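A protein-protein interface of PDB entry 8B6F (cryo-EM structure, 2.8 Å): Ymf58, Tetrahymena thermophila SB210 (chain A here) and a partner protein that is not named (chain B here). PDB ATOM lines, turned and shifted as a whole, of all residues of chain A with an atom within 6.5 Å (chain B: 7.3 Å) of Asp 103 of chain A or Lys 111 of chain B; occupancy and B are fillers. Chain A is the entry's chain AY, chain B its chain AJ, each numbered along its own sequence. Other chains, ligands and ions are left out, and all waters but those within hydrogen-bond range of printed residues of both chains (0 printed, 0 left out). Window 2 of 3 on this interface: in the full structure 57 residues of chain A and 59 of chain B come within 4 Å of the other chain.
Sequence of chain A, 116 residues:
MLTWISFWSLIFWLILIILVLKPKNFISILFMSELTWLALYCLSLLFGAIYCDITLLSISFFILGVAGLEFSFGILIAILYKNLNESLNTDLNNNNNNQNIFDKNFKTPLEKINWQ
Leu 92 of chain A touches Leu 110 of chain B (CD1 to CD1, 3.9 Å). Asn 100 of chain A touches Lys 111 of chain B. Asn 100 of chain A touches Tyr 112 of chain B. Leu 110 of chain B touches Ile 101 of chain A (CD1 to CG2, 3.95 Å). Lys 111 of chain B touches Ile 101 of chain A. Phe 102 of chain A touches Tyr 112 of chain B (CE1 to C, 3.9 Å). Phe 102 of chain A touches Asn 113 of chain B (CE1 to CB, 3.8 Å).
Of chain B, only Lys 111 (3.0 Å) comes within 4 Å of Asp 103 of chain A. Lys 111 of chain B touches just these residues of chain A: Asn 100 (3.6 Å), Ile 101 (3.3 Å), Phe 102 (3.2 Å) and Asp 103 (3.0 Å). Printed residues of chain B within 4 Å of Phe 102 of chain A: Lys 111 (3.2 Å), Tyr 112 (3.9 Å) and Asn 113 (3.8 Å). Printed residues of chain B within 4 Å of Asn 100 of chain A: Lys 111, Tyr 112 and Asn 113. Of the printed residues of chain A, Tyr 112 of chain B touches Asn 100 (3.3 Å) and Phe 102 (3.9 Å). Leu 108 of chain B touches none of the printed residues of chain A. Asn 105 of chain A touches none of the printed residues of chain B. The nearest residue of chain B that does not touch Asp 103 of chain A is Leu 110 of chain B (4.7 Å). The nearest printed residue of chain A that does not touch Lys 111 of chain B is Lys 104 of chain A (6.8 Å). The nearest printed residue of chain A that does not touch Tyr 112 of chain B is Ile 101 of chain A (4.3 Å).
The backbone NH (N) of Phe 102 of chain A is in hydrogen-bond range of the backbone carbonyl oxygen (O) of Lys 111 of chain B (3.2 Å). NZ of Lys 111 of chain B lies within salt-bridge range of OD2 of Asp 103 of chain A (3.0 Å). N of Asn 113 of chain B lies within hydrogen-bond range of O of Asn 100 of chain A.
Of the 7 printed residues of chain A, 5 touch a printed residue of chain B. Of the 7 printed residues of chain B, 4 touch a printed residue of chain A. Hydrophobic or aromatic side chains of chain B that line the printed part of chain A: Leu 110 and Tyr 112. Among the printed residues, 10 pairs touch across the chains.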
ATOM      1  N   LEU A  92      -4.286 -31.718  28.063  1.00  0.00           N
ATOM      2  CA  LEU A  92      -5.322 -31.905  27.057  1.00  0.00           C
ATOM      3  C   LEU A  92      -6.631 -32.417  27.640  1.00  0.00           C
ATOM      4  O   LEU A  92      -7.583 -32.635  26.885  1.00  0.00           O
ATOM      5  CB  LEU A  92      -4.838 -32.875  25.973  1.00  0.00           C
ATOM      6  CG  LEU A  92      -3.676 -32.413  25.090  1.00  0.00           C
ATOM      7  CD1 LEU A  92      -3.289 -33.515  24.122  1.00  0.00           C
ATOM      8  CD2 LEU A  92      -4.023 -31.141  24.334  1.00  0.00           C
ATOM      9  N   ASN A 100       1.202 -22.471  25.812  1.00  0.00           N
ATOM     10  CA  ASN A 100       2.332 -23.389  25.762  1.00  0.00           C
ATOM     11  C   ASN A 100       2.123 -24.527  24.776  1.00  0.00           C
ATOM     12  O   ASN A 100       3.084 -25.241  24.472  1.00  0.00           O
ATOM     13  CB  ASN A 100       2.595 -23.965  27.154  1.00  0.00           C
ATOM     14  CG  ASN A 100       2.942 -22.899  28.168  1.00  0.00           C
ATOM     15  OD1 ASN A 100       4.114 -22.626  28.420  1.00  0.00           O
ATOM     16  ND2 ASN A 100       1.923 -22.289  28.760  1.00  0.00           N
ATOM     17  N   ILE A 101       0.907 -24.711  24.268  1.00  0.00           N
ATOM     18  CA  ILE A 101       0.580 -25.799  23.355  1.00  0.00           C
ATOM     19  C   ILE A 101       0.256 -25.197  21.997  1.00  0.00           C
ATOM     20  O   ILE A 101      -0.590 -24.301  21.892  1.00  0.00           O
ATOM     21  CB  ILE A 101      -0.591 -26.643  23.887  1.00  0.00           C
ATOM     22  CG1 ILE A 101      -0.219 -27.249  25.241  1.00  0.00           C
ATOM     23  CG2 ILE A 101      -0.952 -27.743  22.898  1.00  0.00           C
ATOM     24  CD1 ILE A 101      -1.377 -27.877  25.968  1.00  0.00           C
ATOM     25  N   PHE A 102       0.932 -25.689  20.960  1.00  0.00           N
ATOM     26  CA  PHE A 102       0.752 -25.132  19.624  1.00  0.00           C
ATOM     27  C   PHE A 102      -0.650 -25.396  19.087  1.00  0.00           C
ATOM     28  O   PHE A 102      -1.256 -24.515  18.468  1.00  0.00           O
ATOM     29  CB  PHE A 102       1.797 -25.711  18.672  1.00  0.00           C
ATOM     30  CG  PHE A 102       3.201 -25.276  18.973  1.00  0.00           C
ATOM     31  CD1 PHE A 102       3.928 -25.886  19.980  1.00  0.00           C
ATOM     32  CD2 PHE A 102       3.802 -24.271  18.235  1.00  0.00           C
ATOM     33  CE1 PHE A 102       5.224 -25.492  20.254  1.00  0.00           C
ATOM     34  CE2 PHE A 102       5.097 -23.873  18.503  1.00  0.00           C
ATOM     35  CZ  PHE A 102       5.808 -24.484  19.513  1.00  0.00           C
ATOM     36  N   ASP A 103      -1.182 -26.594  19.314  1.00  0.00           N
ATOM     37  CA  ASP A 103      -2.353 -27.087  18.594  1.00  0.00           C
ATOM     38  C   ASP A 103      -3.424 -27.586  19.555  1.00  0.00           C
ATOM     39  O   ASP A 103      -3.991 -28.666  19.382  1.00  0.00           O
ATOM     40  CB  ASP A 103      -1.957 -28.199  17.628  1.00  0.00           C
ATOM     41  CG  ASP A 103      -1.390 -29.411  18.338  1.00  0.00           C
ATOM     42  OD1 ASP A 103      -0.833 -29.248  19.443  1.00  0.00           O
ATOM     43  OD2 ASP A 103      -1.501 -30.527  17.790  1.00  0.00           O
ATOM     44  N   LYS A 104      -3.724 -26.804  20.587  1.00  0.00           N
ATOM     45  CA  LYS A 104      -4.828 -27.116  21.486  1.00  0.00           C
ATOM     46  C   LYS A 104      -6.082 -26.414  20.978  1.00  0.00           C
ATOM     47  O   LYS A 104      -6.128 -25.181  20.919  1.00  0.00           O
ATOM     48  CB  LYS A 104      -4.510 -26.690  22.918  1.00  0.00           C
ATOM     49  CG  LYS A 104      -5.547 -27.146  23.936  1.00  0.00           C
ATOM     50  CD  LYS A 104      -5.096 -26.856  25.358  1.00  0.00           C
ATOM     51  CE  LYS A 104      -6.123 -27.335  26.372  1.00  0.00           C
ATOM     52  NZ  LYS A 104      -5.681 -27.085  27.772  1.00  0.00           N
ATOM     53  N   ASN A 105      -7.088 -27.199  20.604  1.00  0.00           N
ATOM     54  CA  ASN A 105      -8.310 -26.652  20.020  1.00  0.00           C
ATOM     55  C   ASN A 105      -9.416 -27.681  20.184  1.00  0.00           C
ATOM     56  O   ASN A 105      -9.315 -28.784  19.639  1.00  0.00           O
ATOM     57  CB  ASN A 105      -8.094 -26.313  18.542  1.00  0.00           C
ATOM     58  CG  ASN A 105      -9.307 -25.665  17.902  1.00  0.00           C
ATOM     59  OD1 ASN A 105     -10.449 -25.982  18.234  1.00  0.00           O
ATOM     60  ND2 ASN A 105      -9.064 -24.753  16.968  1.00  0.00           N
ATOM     61  N   ASN B  53      11.090 -33.363  25.029  1.00  0.00           N
ATOM     62  CA  ASN B  53       9.758 -33.848  25.348  1.00  0.00           C
ATOM     63  C   ASN B  53       9.520 -35.279  24.897  1.00  0.00           C
ATOM     64  O   ASN B  53       8.541 -35.893  25.334  1.00  0.00           O
ATOM     65  CB  ASN B  53       8.696 -32.940  24.713  1.00  0.00           C
ATOM     66  CG  ASN B  53       8.660 -31.563  25.337  1.00  0.00           C
ATOM     67  OD1 ASN B  53       8.953 -31.399  26.521  1.00  0.00           O
ATOM     68  ND2 ASN B  53       8.301 -30.563  24.544  1.00  0.00           N
ATOM     69  N   LEU B 108       5.489 -39.843  19.156  1.00  0.00           N
ATOM     70  CA  LEU B 108       4.985 -38.490  18.977  1.00  0.00           C
ATOM     71  C   LEU B 108       4.486 -37.945  20.307  1.00  0.00           C
ATOM     72  O   LEU B 108       3.720 -38.606  21.014  1.00  0.00           O
ATOM     73  CB  LEU B 108       3.863 -38.476  17.940  1.00  0.00           C
ATOM     74  CG  LEU B 108       4.195 -39.106  16.584  1.00  0.00           C
ATOM     75  CD1 LEU B 108       2.986 -39.055  15.667  1.00  0.00           C
ATOM     76  CD2 LEU B 108       5.387 -38.425  15.931  1.00  0.00           C
ATOM     77  N   HIS B 109       4.917 -36.734  20.642  1.00  0.00           N
ATOM     78  CA  HIS B 109       4.631 -36.119  21.926  1.00  0.00           C
ATOM     79  C   HIS B 109       3.835 -34.838  21.723  1.00  0.00           C
ATOM     80  O   HIS B 109       3.637 -34.368  20.600  1.00  0.00           O
ATOM     81  CB  HIS B 109       5.928 -35.822  22.687  1.00  0.00           C
ATOM     82  CG  HIS B 109       6.887 -34.964  21.924  1.00  0.00           C
ATOM     83  ND1 HIS B 109       6.646 -33.633  21.659  1.00  0.00           N
ATOM     84  CD2 HIS B 109       8.085 -35.247  21.362  1.00  0.00           C
ATOM     85  CE1 HIS B 109       7.655 -33.134  20.969  1.00  0.00           C
ATOM     86  NE2 HIS B 109       8.542 -34.092  20.775  1.00  0.00           N
ATOM     87  N   LEU B 110       3.382 -34.273  22.838  1.00  0.00           N
ATOM     88  CA  LEU B 110       2.651 -33.016  22.792  1.00  0.00           C
ATOM     89  C   LEU B 110       3.543 -31.902  22.263  1.00  0.00           C
ATOM     90  O   LEU B 110       4.735 -31.836  22.574  1.00  0.00           O
ATOM     91  CB  LEU B 110       2.134 -32.659  24.187  1.00  0.00           C
ATOM     92  CG  LEU B 110       1.296 -31.386  24.297  1.00  0.00           C
ATOM     93  CD1 LEU B 110      -0.001 -31.529  23.523  1.00  0.00           C
ATOM     94  CD2 LEU B 110       1.021 -31.061  25.751  1.00  0.00           C
ATOM     95  N   LYS B 111       2.958 -31.024  21.453  1.00  0.00           N
ATOM     96  CA  LYS B 111       3.671 -29.872  20.906  1.00  0.00           C
ATOM     97  C   LYS B 111       3.694 -28.796  21.981  1.00  0.00           C
ATOM     98  O   LYS B 111       2.765 -28.001  22.121  1.00  0.00           O
ATOM     99  CB  LYS B 111       3.006 -29.381  19.628  1.00  0.00           C
ATOM    100  CG  LYS B 111       2.829 -30.464  18.577  1.00  0.00           C
ATOM    101  CD  LYS B 111       2.097 -29.932  17.360  1.00  0.00           C
ATOM    102  CE  LYS B 111       1.800 -31.038  16.365  1.00  0.00           C
ATOM    103  NZ  LYS B 111       0.929 -32.096  16.943  1.00  0.00           N
ATOM    104  N   TYR B 112       4.777 -28.771  22.749  1.00  0.00           N
ATOM    105  CA  TYR B 112       4.900 -27.919  23.920  1.00  0.00           C
ATOM    106  C   TYR B 112       6.058 -26.949  23.733  1.00  0.00           C
ATOM    107  O   TYR B 112       7.138 -27.337  23.278  1.00  0.00           O
ATOM    108  CB  TYR B 112       5.119 -28.759  25.179  1.00  0.00           C
ATOM    109  CG  TYR B 112       4.920 -28.003  26.467  1.00  0.00           C
ATOM    110  CD1 TYR B 112       3.651 -27.846  27.011  1.00  0.00           C
ATOM    111  CD2 TYR B 112       5.998 -27.457  27.148  1.00  0.00           C
ATOM    112  CE1 TYR B 112       3.462 -27.160  28.191  1.00  0.00           C
ATOM    113  CE2 TYR B 112       5.818 -26.770  28.330  1.00  0.00           C
ATOM    114  CZ  TYR B 112       4.548 -26.625  28.846  1.00  0.00           C
ATOM    115  OH  TYR B 112       4.366 -25.941  30.024  1.00  0.00           O
ATOM    116  N   ASN B 113       5.820 -25.687  24.079  1.00  0.00           N
ATOM    117  CA  ASN B 113       6.829 -24.636  24.012  1.00  0.00           C
ATOM    118  C   ASN B 113       7.209 -24.255  25.437  1.00  0.00           C
ATOM    119  O   ASN B 113       6.409 -23.649  26.158  1.00  0.00           O
ATOM    120  CB  ASN B 113       6.306 -23.430  23.236  1.00  0.00           C
ATOM    121  CG  ASN B 113       7.355 -22.356  23.056  1.00  0.00           C
ATOM    122  OD1 ASN B 113       8.539 -22.585  23.299  1.00  0.00           O
ATOM    123  ND2 ASN B 113       6.929 -21.179  22.623  1.00  0.00           N
